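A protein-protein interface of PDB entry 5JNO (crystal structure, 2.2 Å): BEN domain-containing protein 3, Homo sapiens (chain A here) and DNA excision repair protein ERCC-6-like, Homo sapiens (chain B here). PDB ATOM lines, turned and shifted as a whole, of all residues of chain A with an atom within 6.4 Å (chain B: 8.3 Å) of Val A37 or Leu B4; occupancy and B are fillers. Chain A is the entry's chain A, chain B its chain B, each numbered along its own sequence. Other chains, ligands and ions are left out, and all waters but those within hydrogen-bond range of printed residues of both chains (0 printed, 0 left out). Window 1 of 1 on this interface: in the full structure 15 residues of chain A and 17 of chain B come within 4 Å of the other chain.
Among the printed residues, merely in contact across the chains: Gln A24 with Ala B1, Gln A24 with Glu B2, Gln A24 with Phe B42, Asp A30 with Ala B3, Arg A34 with Leu B4, Arg A34 with Phe B42, Val A37 with Leu B4, Val A37 with Ala B9, Gln A38 with Phe B42, Pro A41 with Leu B13, Phe A44 with Leu B13, Phe A100 with Leu B4, Phe A100 with Ser B5, Phe A100 with Pro B6, Phe A100 with Ala B9 and Arg A103 with Pro B6.
The side-chain hydroxyl of Ser B5 sits at hydrogen-bond distance from the backbone NH of Gln B8.
The side-chain amide oxygen (OD1) of Asn B44 lies close to the backbone carbonyl oxygen (O) of Phe B42 (3.0 Å).
The side-chain hydroxyl (OG) of Ser B5 lies close to the backbone NH (N) of Glu B7, at 3.4 Å.
The backbone carbonyl oxygen (O) of Gln A24 lies within hydrogen-bond range of the guanidinium group (NH2) of Arg A34 (3.4 Å).
The backbone carbonyl oxygen (O) of Ala B3 sits close to the side-chain amide oxygen (OE1) of Gln B8 (3.4 Å).
The side-chain carboxylate of Asp A30 lies within salt-bridge range of the guanidinium group of Arg A34 (2.9 Å).
Of chain B, only Leu B4 and Ala B9 come within 4 Å of Val A37.
Of chain A, only Asp A30 (2.9 Å), Arg A34 (3.6 Å), Val A37 (3.9 Å) and Phe A100 (3.4 Å) come within 4 Å of Leu B4.
Of the printed residues of chain A, Pro B43 touches Gln A24 (3.1 Å).
Printed residues of chain A within 4 Å of Asn B44: Gln A38 (3.3 Å).
His B11 touches none of the printed residues of chain A.
The nearest printed residue of chain B that does not touch Val A37 is Leu B13 (4.04 Å).
The nearest printed residue of chain B that does not touch Phe A100 is Glu B7 (6.0 Å).
The side-chain amide nitrogen (NE2) of Gln A38 is in hydrogen-bond range of the side-chain amide oxygen (OD1) of Asn B44.
OE1 of Gln A24 lies close to O of Pro B43.
O of Glu B2 sits close to OD2 of Asp A30, 3.5 Å away.
The backbone NH of Leu B4 is in hydrogen-bond range of the side-chain carboxylate of Asp A30, at 2.9 Å.
The side-chain hydroxyl of Tyr B12 is in hydrogen-bond range of the side-chain amide nitrogen of Gln A38.
OE1 of Glu B7 is in salt-bridge range of NH2 of Arg A103 (3.9 Å).
O of Glu B2 is in hydrogen-bond range of NH2 of Arg A34 (2.8 Å).
Printed residues of chain B that touch a printed residue of chain A: Ala B1, Glu B2, Ala B3, Leu B4, Ser B5, Pro B6, Glu B7, Ala B9, Tyr B12, Leu B13, Phe B42, Pro B43 and Asn B44.
Hydrophobic or aromatic side chains of chain B within 4 Å of the printed part of chain A: Ala B3, Leu B4, Pro B6, Ala B9, Tyr B12, Leu B13, Phe B42 and Pro B43.
Of the 17 printed residues of chain A, 9 touch a printed residue of chain B.
Hydrophobic or aromatic side chains of chain A within 4 Å of the printed part of chain B: Val A37, Pro A41, Phe A44 and Phe A100.
Among the printed residues, Asp or Glu carboxylates within 4 Å of a Lys or Arg side-chain nitrogen of the other chain: Arg A103 with Glu B7.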
ATOM      1  N   GLN A  24     -29.775 -24.017 -25.309  1.00  0.00           N
ATOM      2  CA  GLN A  24     -30.300 -24.309 -23.967  1.00  0.00           C
ATOM      3  C   GLN A  24     -30.424 -23.052 -23.099  1.00  0.00           C
ATOM      4  O   GLN A  24     -30.972 -23.120 -22.004  1.00  0.00           O
ATOM      5  CB  GLN A  24     -29.391 -25.290 -23.241  1.00  0.00           C
ATOM      6  CG  GLN A  24     -29.269 -26.648 -23.883  1.00  0.00           C
ATOM      7  CD  GLN A  24     -27.938 -27.279 -23.553  1.00  0.00           C
ATOM      8  OE1 GLN A  24     -27.826 -28.016 -22.593  1.00  0.00           O
ATOM      9  NE2 GLN A  24     -26.910 -26.938 -24.316  1.00  0.00           N
ATOM     10  N   ASP A  30     -27.915 -16.102 -18.810  1.00  0.00           N
ATOM     11  CA  ASP A  30     -27.862 -17.527 -18.571  1.00  0.00           C
ATOM     12  C   ASP A  30     -26.809 -18.153 -19.471  1.00  0.00           C
ATOM     13  O   ASP A  30     -26.040 -18.998 -19.018  1.00  0.00           O
ATOM     14  CB  ASP A  30     -29.217 -18.173 -18.824  1.00  0.00           C
ATOM     15  CG  ASP A  30     -29.202 -19.685 -18.573  1.00  0.00           C
ATOM     16  OD1 ASP A  30     -28.562 -20.144 -17.585  1.00  0.00           O
ATOM     17  OD2 ASP A  30     -29.863 -20.412 -19.368  1.00  0.00           O
ATOM     18  N   ALA A  32     -24.173 -16.643 -20.467  1.00  0.00           N
ATOM     19  CA  ALA A  32     -22.911 -16.327 -19.853  1.00  0.00           C
ATOM     20  C   ALA A  32     -22.548 -17.293 -18.698  1.00  0.00           C
ATOM     21  O   ALA A  32     -21.407 -17.716 -18.606  1.00  0.00           O
ATOM     22  CB  ALA A  32     -22.869 -14.884 -19.398  1.00  0.00           C
ATOM     23  N   CYS A  33     -23.507 -17.623 -17.842  1.00  0.00           N
ATOM     24  CA  CYS A  33     -23.268 -18.543 -16.748  1.00  0.00           C
ATOM     25  C   CYS A  33     -22.975 -19.976 -17.250  1.00  0.00           C
ATOM     26  O   CYS A  33     -22.109 -20.627 -16.727  1.00  0.00           O
ATOM     27  CB  CYS A  33     -24.444 -18.512 -15.764  1.00  0.00           C
ATOM     28  SG  CYS A  33     -24.736 -16.835 -15.030  1.00  0.00           S
ATOM     29  N   ARG A  34     -23.678 -20.438 -18.273  1.00  0.00           N
ATOM     30  CA  ARG A  34     -23.398 -21.760 -18.868  1.00  0.00           C
ATOM     31  C   ARG A  34     -22.011 -21.828 -19.458  1.00  0.00           C
ATOM     32  O   ARG A  34     -21.299 -22.805 -19.241  1.00  0.00           O
ATOM     33  CB  ARG A  34     -24.390 -22.092 -19.939  1.00  0.00           C
ATOM     34  CG  ARG A  34     -25.745 -22.353 -19.357  1.00  0.00           C
ATOM     35  CD  ARG A  34     -26.786 -22.352 -20.468  1.00  0.00           C
ATOM     36  NE  ARG A  34     -28.077 -22.680 -19.908  1.00  0.00           N
ATOM     37  CZ  ARG A  34     -28.441 -23.890 -19.516  1.00  0.00           C
ATOM     38  NH1 ARG A  34     -27.616 -24.936 -19.651  1.00  0.00           N
ATOM     39  NH2 ARG A  34     -29.654 -24.055 -19.001  1.00  0.00           N
ATOM     40  N   LEU A  35     -21.626 -20.754 -20.149  1.00  0.00           N
ATOM     41  CA  LEU A  35     -20.304 -20.631 -20.654  1.00  0.00           C
ATOM     42  C   LEU A  35     -19.262 -20.624 -19.528  1.00  0.00           C
ATOM     43  O   LEU A  35     -18.203 -21.204 -19.686  1.00  0.00           O
ATOM     44  CB  LEU A  35     -20.162 -19.396 -21.550  1.00  0.00           C
ATOM     45  CG  LEU A  35     -20.812 -19.394 -22.941  1.00  0.00           C
ATOM     46  CD1 LEU A  35     -20.896 -17.967 -23.485  1.00  0.00           C
ATOM     47  CD2 LEU A  35     -20.006 -20.241 -23.904  1.00  0.00           C
ATOM     48  N   LEU A  36     -19.528 -19.975 -18.404  1.00  0.00           N
ATOM     49  CA  LEU A  36     -18.566 -20.003 -17.292  1.00  0.00           C
ATOM     50  C   LEU A  36     -18.279 -21.467 -16.822  1.00  0.00           C
ATOM     51  O   LEU A  36     -17.149 -21.872 -16.567  1.00  0.00           O
ATOM     52  CB  LEU A  36     -19.115 -19.169 -16.143  1.00  0.00           C
ATOM     53  CG  LEU A  36     -18.361 -19.120 -14.832  1.00  0.00           C
ATOM     54  CD1 LEU A  36     -16.971 -18.529 -14.989  1.00  0.00           C
ATOM     55  CD2 LEU A  36     -19.148 -18.370 -13.752  1.00  0.00           C
ATOM     56  N   VAL A  37     -19.354 -22.225 -16.719  1.00  0.00           N
ATOM     57  CA  VAL A  37     -19.340 -23.580 -16.276  1.00  0.00           C
ATOM     58  C   VAL A  37     -18.599 -24.460 -17.266  1.00  0.00           C
ATOM     59  O   VAL A  37     -17.712 -25.182 -16.850  1.00  0.00           O
ATOM     60  CB  VAL A  37     -20.768 -24.074 -16.036  1.00  0.00           C
ATOM     61  CG1 VAL A  37     -20.822 -25.597 -15.839  1.00  0.00           C
ATOM     62  CG2 VAL A  37     -21.334 -23.345 -14.837  1.00  0.00           C
ATOM     63  N   GLN A  38     -18.902 -24.338 -18.555  1.00  0.00           N
ATOM     64  CA  GLN A  38     -18.228 -25.131 -19.591  1.00  0.00           C
ATOM     65  C   GLN A  38     -16.801 -24.749 -19.807  1.00  0.00           C
ATOM     66  O   GLN A  38     -15.980 -25.604 -20.002  1.00  0.00           O
ATOM     67  CB  GLN A  38     -18.925 -24.988 -20.938  1.00  0.00           C
ATOM     68  CG  GLN A  38     -20.235 -25.731 -21.015  1.00  0.00           C
ATOM     69  CD  GLN A  38     -20.040 -27.238 -21.121  1.00  0.00           C
ATOM     70  OE1 GLN A  38     -19.179 -27.706 -21.837  1.00  0.00           O
ATOM     71  NE2 GLN A  38     -20.830 -27.985 -20.385  1.00  0.00           N
ATOM     72  N   LEU A  39     -16.480 -23.453 -19.840  1.00  0.00           N
ATOM     73  CA  LEU A  39     -15.090 -23.068 -20.148  1.00  0.00           C
ATOM     74  C   LEU A  39     -14.164 -23.233 -18.976  1.00  0.00           C
ATOM     75  O   LEU A  39     -13.011 -23.573 -19.177  1.00  0.00           O
ATOM     76  CB  LEU A  39     -15.036 -21.622 -20.611  1.00  0.00           C
ATOM     77  CG  LEU A  39     -15.711 -21.393 -21.953  1.00  0.00           C
ATOM     78  CD1 LEU A  39     -15.884 -19.907 -22.088  1.00  0.00           C
ATOM     79  CD2 LEU A  39     -14.864 -21.987 -23.076  1.00  0.00           C
ATOM     80  N   PHE A  40     -14.647 -22.957 -17.755  1.00  0.00           N
ATOM     81  CA  PHE A  40     -13.766 -22.729 -16.586  1.00  0.00           C
ATOM     82  C   PHE A  40     -14.159 -23.536 -15.363  1.00  0.00           C
ATOM     83  O   PHE A  40     -14.279 -22.985 -14.259  1.00  0.00           O
ATOM     84  CB  PHE A  40     -13.722 -21.224 -16.203  1.00  0.00           C
ATOM     85  CG  PHE A  40     -13.312 -20.326 -17.311  1.00  0.00           C
ATOM     86  CD1 PHE A  40     -12.150 -20.574 -18.024  1.00  0.00           C
ATOM     87  CD2 PHE A  40     -14.084 -19.206 -17.652  1.00  0.00           C
ATOM     88  CE1 PHE A  40     -11.768 -19.724 -19.053  1.00  0.00           C
ATOM     89  CE2 PHE A  40     -13.709 -18.369 -18.688  1.00  0.00           C
ATOM     90  CZ  PHE A  40     -12.544 -18.616 -19.372  1.00  0.00           C
ATOM     91  N   PRO A  41     -14.267 -24.866 -15.516  1.00  0.00           N
ATOM     92  CA  PRO A  41     -14.645 -25.659 -14.369  1.00  0.00           C
ATOM     93  C   PRO A  41     -13.617 -25.633 -13.240  1.00  0.00           C
ATOM     94  O   PRO A  41     -14.003 -25.801 -12.068  1.00  0.00           O
ATOM     95  CB  PRO A  41     -14.782 -27.095 -14.969  1.00  0.00           C
ATOM     96  CG  PRO A  41     -13.822 -27.117 -16.139  1.00  0.00           C
ATOM     97  CD  PRO A  41     -14.005 -25.709 -16.710  1.00  0.00           C
ATOM     98  N   GLU A  42     -12.337 -25.447 -13.567  1.00  0.00           N
ATOM     99  CA  GLU A  42     -11.295 -25.197 -12.551  1.00  0.00           C
ATOM    100  C   GLU A  42     -11.641 -24.059 -11.538  1.00  0.00           C
ATOM    101  O   GLU A  42     -11.237 -24.136 -10.389  1.00  0.00           O
ATOM    102  CB  GLU A  42      -9.917 -24.923 -13.190  1.00  0.00           C
ATOM    103  CG  GLU A  42      -9.733 -23.597 -13.965  1.00  0.00           C
ATOM    104  CD  GLU A  42     -10.195 -23.663 -15.412  1.00  0.00           C
ATOM    105  OE1 GLU A  42     -10.963 -24.576 -15.776  1.00  0.00           O
ATOM    106  OE2 GLU A  42      -9.791 -22.808 -16.213  1.00  0.00           O
ATOM    107  N   PHE A  44     -14.367 -23.618 -10.114  1.00  0.00           N
ATOM    108  CA  PHE A  44     -15.317 -24.161  -9.145  1.00  0.00           C
ATOM    109  C   PHE A  44     -14.751 -25.228  -8.222  1.00  0.00           C
ATOM    110  O   PHE A  44     -15.477 -25.746  -7.398  1.00  0.00           O
ATOM    111  CB  PHE A  44     -16.550 -24.693  -9.865  1.00  0.00           C
ATOM    112  CG  PHE A  44     -17.266 -23.654 -10.697  1.00  0.00           C
ATOM    113  CD1 PHE A  44     -16.819 -23.324 -11.965  1.00  0.00           C
ATOM    114  CD2 PHE A  44     -18.393 -23.010 -10.211  1.00  0.00           C
ATOM    115  CE1 PHE A  44     -17.485 -22.392 -12.725  1.00  0.00           C
ATOM    116  CE2 PHE A  44     -19.068 -22.073 -10.969  1.00  0.00           C
ATOM    117  CZ  PHE A  44     -18.600 -21.755 -12.237  1.00  0.00           C
ATOM    118  N   ILE A  72     -15.709 -14.960 -22.144  1.00  0.00           N
ATOM    119  CA  ILE A  72     -17.135 -15.274 -22.094  1.00  0.00           C
ATOM    120  C   ILE A  72     -17.963 -14.252 -22.889  1.00  0.00           C
ATOM    121  O   ILE A  72     -18.851 -14.624 -23.653  1.00  0.00           O
ATOM    122  CB  ILE A  72     -17.652 -15.314 -20.647  1.00  0.00           C
ATOM    123  CG1 ILE A  72     -17.050 -16.520 -19.903  1.00  0.00           C
ATOM    124  CG2 ILE A  72     -19.186 -15.355 -20.604  1.00  0.00           C
ATOM    125  CD1 ILE A  72     -17.228 -16.454 -18.390  1.00  0.00           C
ATOM    126  N   PHE A 100     -24.209 -15.625  -9.821  1.00  0.00           N
ATOM    127  CA  PHE A 100     -24.066 -17.083 -10.012  1.00  0.00           C
ATOM    128  C   PHE A 100     -22.858 -17.625  -9.253  1.00  0.00           C
ATOM    129  O   PHE A 100     -22.969 -18.520  -8.425  1.00  0.00           O
ATOM    130  CB  PHE A 100     -23.913 -17.380 -11.494  1.00  0.00           C
ATOM    131  CG  PHE A 100     -23.886 -18.854 -11.835  1.00  0.00           C
ATOM    132  CD1 PHE A 100     -25.065 -19.548 -12.051  1.00  0.00           C
ATOM    133  CD2 PHE A 100     -22.686 -19.542 -11.931  1.00  0.00           C
ATOM    134  CE1 PHE A 100     -25.048 -20.921 -12.353  1.00  0.00           C
ATOM    135  CE2 PHE A 100     -22.659 -20.913 -12.232  1.00  0.00           C
ATOM    136  CZ  PHE A 100     -23.846 -21.597 -12.444  1.00  0.00           C
ATOM    137  N   ARG A 103     -23.178 -17.210  -5.450  1.00  0.00           N
ATOM    138  CA  ARG A 103     -24.144 -18.204  -4.956  1.00  0.00           C
ATOM    139  C   ARG A 103     -23.536 -19.606  -4.901  1.00  0.00           C
ATOM    140  O   ARG A 103     -23.670 -20.303  -3.916  1.00  0.00           O
ATOM    141  CB  ARG A 103     -25.412 -18.196  -5.814  1.00  0.00           C
ATOM    142  CG  ARG A 103     -26.303 -16.974  -5.550  1.00  0.00           C
ATOM    143  CD  ARG A 103     -27.474 -16.878  -6.517  1.00  0.00           C
ATOM    144  NE  ARG A 103     -28.369 -18.006  -6.277  1.00  0.00           N
ATOM    145  CZ  ARG A 103     -29.185 -18.573  -7.172  1.00  0.00           C
ATOM    146  NH1 ARG A 103     -29.270 -18.115  -8.428  1.00  0.00           N
ATOM    147  NH2 ARG A 103     -29.934 -19.614  -6.794  1.00  0.00           N
ATOM    148  N   ALA B   1     -36.139 -23.435 -22.551  1.00  0.00           N
ATOM    149  CA  ALA B   1     -36.001 -24.486 -21.523  1.00  0.00           C
ATOM    150  C   ALA B   1     -34.850 -24.163 -20.535  1.00  0.00           C
ATOM    151  O   ALA B   1     -33.752 -24.751 -20.621  1.00  0.00           O
ATOM    152  CB  ALA B   1     -35.815 -25.859 -22.180  1.00  0.00           C
ATOM    153  N   GLU B   2     -35.104 -23.189 -19.646  1.00  0.00           N
ATOM    154  CA  GLU B   2     -34.586 -23.180 -18.243  1.00  0.00           C
ATOM    155  C   GLU B   2     -33.165 -22.612 -17.990  1.00  0.00           C
ATOM    156  O   GLU B   2     -32.215 -22.919 -18.732  1.00  0.00           O
ATOM    157  CB  GLU B   2     -34.700 -24.609 -17.662  1.00  0.00           C
ATOM    158  CG  GLU B   2     -34.797 -24.757 -16.144  1.00  0.00           C
ATOM    159  CD  GLU B   2     -35.262 -26.162 -15.745  1.00  0.00           C
ATOM    160  OE1 GLU B   2     -36.420 -26.526 -16.055  1.00  0.00           O
ATOM    161  OE2 GLU B   2     -34.470 -26.911 -15.135  1.00  0.00           O
ATOM    162  N   ALA B   3     -33.034 -21.806 -16.923  1.00  0.00           N
ATOM    163  CA  ALA B   3     -31.735 -21.227 -16.516  1.00  0.00           C
ATOM    164  C   ALA B   3     -30.950 -22.210 -15.678  1.00  0.00           C
ATOM    165  O   ALA B   3     -31.524 -22.889 -14.827  1.00  0.00           O
ATOM    166  CB  ALA B   3     -31.921 -19.923 -15.741  1.00  0.00           C
ATOM    167  N   LEU B   4     -29.644 -22.299 -15.905  1.00  0.00           N
ATOM    168  CA  LEU B   4     -28.811 -23.171 -15.079  1.00  0.00           C
ATOM    169  C   LEU B   4     -28.668 -22.548 -13.693  1.00  0.00           C
ATOM    170  O   LEU B   4     -28.154 -21.435 -13.575  1.00  0.00           O
ATOM    171  CB  LEU B   4     -27.416 -23.352 -15.692  1.00  0.00           C
ATOM    172  CG  LEU B   4     -26.478 -24.349 -14.981  1.00  0.00           C
ATOM    173  CD1 LEU B   4     -26.929 -25.806 -15.091  1.00  0.00           C
ATOM    174  CD2 LEU B   4     -25.084 -24.221 -15.560  1.00  0.00           C
ATOM    175  N   SER B   5     -29.123 -23.264 -12.674  1.00  0.00           N
ATOM    176  CA  SER B   5     -28.969 -22.867 -11.277  1.00  0.00           C
ATOM    177  C   SER B   5     -27.579 -23.230 -10.772  1.00  0.00           C
ATOM    178  O   SER B   5     -26.943 -24.138 -11.285  1.00  0.00           O
ATOM    179  CB  SER B   5     -30.027 -23.556 -10.401  1.00  0.00           C
ATOM    180  OG  SER B   5     -29.657 -24.895 -10.117  1.00  0.00           O
ATOM    181  N   PRO B   6     -27.096 -22.534  -9.746  1.00  0.00           N
ATOM    182  CA  PRO B   6     -25.813 -22.922  -9.194  1.00  0.00           C
ATOM    183  C   PRO B   6     -25.788 -24.337  -8.603  1.00  0.00           C
ATOM    184  O   PRO B   6     -24.740 -24.963  -8.570  1.00  0.00           O
ATOM    185  CB  PRO B   6     -25.578 -21.879  -8.111  1.00  0.00           C
ATOM    186  CG  PRO B   6     -26.322 -20.679  -8.596  1.00  0.00           C
ATOM    187  CD  PRO B   6     -27.559 -21.236  -9.211  1.00  0.00           C
ATOM    188  N   GLU B   7     -26.942 -24.799  -8.134  1.00  0.00           N
ATOM    189  CA  GLU B   7     -27.134 -26.156  -7.634  1.00  0.00           C
ATOM    190  C   GLU B   7     -26.927 -27.162  -8.740  1.00  0.00           C
ATOM    191  O   GLU B   7     -26.209 -28.128  -8.571  1.00  0.00           O
ATOM    192  CB  GLU B   7     -28.562 -26.347  -7.077  1.00  0.00           C
ATOM    193  CG  GLU B   7     -28.897 -25.525  -5.839  1.00  0.00           C
ATOM    194  CD  GLU B   7     -29.572 -24.177  -6.131  1.00  0.00           C
ATOM    195  OE1 GLU B   7     -29.106 -23.378  -6.984  1.00  0.00           O
ATOM    196  OE2 GLU B   7     -30.584 -23.908  -5.480  1.00  0.00           O
ATOM    197  N   GLN B   8     -27.574 -26.925  -9.870  1.00  0.00           N
ATOM    198  CA  GLN B   8     -27.390 -27.761 -11.038  1.00  0.00           C
ATOM    199  C   GLN B   8     -25.922 -27.778 -11.473  1.00  0.00           C
ATOM    200  O   GLN B   8     -25.354 -28.847 -11.668  1.00  0.00           O
ATOM    201  CB  GLN B   8     -28.286 -27.292 -12.179  1.00  0.00           C
ATOM    202  CG  GLN B   8     -29.756 -27.585 -11.937  1.00  0.00           C
ATOM    203  CD  GLN B   8     -30.689 -26.960 -12.979  1.00  0.00           C
ATOM    204  OE1 GLN B   8     -30.500 -25.830 -13.451  1.00  0.00           O
ATOM    205  NE2 GLN B   8     -31.728 -27.702 -13.330  1.00  0.00           N
ATOM    206  N   ALA B   9     -25.302 -26.600 -11.579  1.00  0.00           N
ATOM    207  CA  ALA B   9     -23.921 -26.520 -12.017  1.00  0.00           C
ATOM    208  C   ALA B   9     -23.035 -27.339 -11.126  1.00  0.00           C
ATOM    209  O   ALA B   9     -22.150 -28.060 -11.619  1.00  0.00           O
ATOM    210  CB  ALA B   9     -23.426 -25.088 -12.080  1.00  0.00           C
ATOM    211  N   ALA B  10     -23.270 -27.235  -9.817  1.00  0.00           N
ATOM    212  CA  ALA B  10     -22.425 -27.930  -8.844  1.00  0.00           C
ATOM    213  C   ALA B  10     -22.502 -29.445  -9.035  1.00  0.00           C
ATOM    214  O   ALA B  10     -21.481 -30.111  -9.022  1.00  0.00           O
ATOM    215  CB  ALA B  10     -22.791 -27.532  -7.420  1.00  0.00           C
ATOM    216  N   HIS B  11     -23.713 -29.955  -9.222  1.00  0.00           N
ATOM    217  CA  HIS B  11     -23.940 -31.379  -9.474  1.00  0.00           C
ATOM    218  C   HIS B  11     -23.333 -31.821 -10.800  1.00  0.00           C
ATOM    219  O   HIS B  11     -22.637 -32.841 -10.849  1.00  0.00           O
ATOM    220  CB  HIS B  11     -25.435 -31.691  -9.469  1.00  0.00           C
ATOM    221  CG  HIS B  11     -26.026 -31.740  -8.100  1.00  0.00           C
ATOM    222  ND1 HIS B  11     -25.528 -32.563  -7.110  1.00  0.00           N
ATOM    223  CD2 HIS B  11     -27.076 -31.089  -7.558  1.00  0.00           C
ATOM    224  CE1 HIS B  11     -26.240 -32.402  -6.011  1.00  0.00           C
ATOM    225  NE2 HIS B  11     -27.178 -31.504  -6.254  1.00  0.00           N
ATOM    226  N   TYR B  12     -23.575 -31.035 -11.856  1.00  0.00           N
ATOM    227  CA  TYR B  12     -22.953 -31.259 -13.149  1.00  0.00           C
ATOM    228  C   TYR B  12     -21.436 -31.375 -13.028  1.00  0.00           C
ATOM    229  O   TYR B  12     -20.843 -32.382 -13.473  1.00  0.00           O
ATOM    230  CB  TYR B  12     -23.326 -30.194 -14.148  1.00  0.00           C
ATOM    231  CG  TYR B  12     -22.574 -30.308 -15.452  1.00  0.00           C
ATOM    232  CD1 TYR B  12     -23.031 -31.147 -16.484  1.00  0.00           C
ATOM    233  CD2 TYR B  12     -21.392 -29.602 -15.662  1.00  0.00           C
ATOM    234  CE1 TYR B  12     -22.325 -31.278 -17.683  1.00  0.00           C
ATOM    235  CE2 TYR B  12     -20.677 -29.734 -16.857  1.00  0.00           C
ATOM    236  CZ  TYR B  12     -21.155 -30.580 -17.865  1.00  0.00           C
ATOM    237  OH  TYR B  12     -20.449 -30.701 -19.035  1.00  0.00           O
ATOM    238  N   LEU B  13     -20.823 -30.389 -12.390  1.00  0.00           N
ATOM    239  CA  LEU B  13     -19.376 -30.373 -12.265  1.00  0.00           C
ATOM    240  C   LEU B  13     -18.800 -31.517 -11.408  1.00  0.00           C
ATOM    241  O   LEU B  13     -17.730 -32.023 -11.709  1.00  0.00           O
ATOM    242  CB  LEU B  13     -18.873 -29.019 -11.762  1.00  0.00           C
ATOM    243  CG  LEU B  13     -19.047 -27.834 -12.741  1.00  0.00           C
ATOM    244  CD1 LEU B  13     -19.002 -26.491 -12.005  1.00  0.00           C
ATOM    245  CD2 LEU B  13     -17.981 -27.836 -13.815  1.00  0.00           C
ATOM    246  N   VAL B  16     -18.991 -34.772 -13.589  1.00  0.00           N
ATOM    247  CA  VAL B  16     -17.919 -34.842 -14.588  1.00  0.00           C
ATOM    248  C   VAL B  16     -16.581 -35.116 -13.925  1.00  0.00           C
ATOM    249  O   VAL B  16     -15.825 -35.935 -14.433  1.00  0.00           O
ATOM    250  CB  VAL B  16     -17.827 -33.561 -15.465  1.00  0.00           C
ATOM    251  CG1 VAL B  16     -16.581 -33.534 -16.349  1.00  0.00           C
ATOM    252  CG2 VAL B  16     -19.068 -33.459 -16.327  1.00  0.00           C
ATOM    253  N   ALA B  38     -24.690 -36.193 -15.584  1.00  0.00           N
ATOM    254  CA  ALA B  38     -24.243 -34.907 -16.130  1.00  0.00           C
ATOM    255  C   ALA B  38     -24.991 -34.475 -17.404  1.00  0.00           C
ATOM    256  O   ALA B  38     -25.483 -33.346 -17.500  1.00  0.00           O
ATOM    257  CB  ALA B  38     -22.746 -34.942 -16.387  1.00  0.00           C
ATOM    258  N   ILE B  41     -28.378 -32.989 -16.801  1.00  0.00           N
ATOM    259  CA  ILE B  41     -28.410 -31.600 -16.331  1.00  0.00           C
ATOM    260  C   ILE B  41     -28.031 -30.645 -17.463  1.00  0.00           C
ATOM    261  O   ILE B  41     -28.722 -29.659 -17.693  1.00  0.00           O
ATOM    262  CB  ILE B  41     -27.455 -31.394 -15.130  1.00  0.00           C
ATOM    263  CG1 ILE B  41     -27.858 -32.318 -13.973  1.00  0.00           C
ATOM    264  CG2 ILE B  41     -27.437 -29.923 -14.692  1.00  0.00           C
ATOM    265  CD1 ILE B  41     -26.851 -32.416 -12.856  1.00  0.00           C
ATOM    266  N   PHE B  42     -26.942 -30.932 -18.169  1.00  0.00           N
ATOM    267  CA  PHE B  42     -26.355 -29.972 -19.118  1.00  0.00           C
ATOM    268  C   PHE B  42     -25.721 -30.735 -20.284  1.00  0.00           C
ATOM    269  O   PHE B  42     -24.507 -30.958 -20.312  1.00  0.00           O
ATOM    270  CB  PHE B  42     -25.320 -29.101 -18.382  1.00  0.00           C
ATOM    271  CG  PHE B  42     -24.794 -27.909 -19.161  1.00  0.00           C
ATOM    272  CD1 PHE B  42     -25.048 -27.709 -20.526  1.00  0.00           C
ATOM    273  CD2 PHE B  42     -23.992 -26.976 -18.500  1.00  0.00           C
ATOM    274  CE1 PHE B  42     -24.545 -26.610 -21.197  1.00  0.00           C
ATOM    275  CE2 PHE B  42     -23.488 -25.858 -19.166  1.00  0.00           C
ATOM    276  CZ  PHE B  42     -23.765 -25.682 -20.517  1.00  0.00           C
ATOM    277  N   PRO B  43     -26.551 -31.120 -21.267  1.00  0.00           N
ATOM    278  CA  PRO B  43     -26.000 -31.936 -22.353  1.00  0.00           C
ATOM    279  C   PRO B  43     -24.998 -31.133 -23.194  1.00  0.00           C
ATOM    280  O   PRO B  43     -25.222 -29.948 -23.408  1.00  0.00           O
ATOM    281  CB  PRO B  43     -27.250 -32.324 -23.174  1.00  0.00           C
ATOM    282  CG  PRO B  43     -28.308 -31.333 -22.799  1.00  0.00           C
ATOM    283  CD  PRO B  43     -28.011 -30.921 -21.392  1.00  0.00           C
ATOM    284  N   ASN B  44     -23.904 -31.761 -23.619  1.00  0.00           N
ATOM    285  CA  ASN B  44     -22.930 -31.122 -24.511  1.00  0.00           C
ATOM    286  C   ASN B  44     -22.059 -32.147 -25.209  1.00  0.00           C
ATOM    287  O   ASN B  44     -21.788 -33.205 -24.658  1.00  0.00           O
ATOM    288  CB  ASN B  44     -22.035 -30.105 -23.764  1.00  0.00           C
ATOM    289  CG  ASN B  44     -21.217 -30.738 -22.635  1.00  0.00           C
ATOM    290  OD1 ASN B  44     -21.730 -30.971 -21.534  1.00  0.00           O
ATOM    291  ND2 ASN B  44     -19.940 -30.996 -22.894  1.00  0.00           N
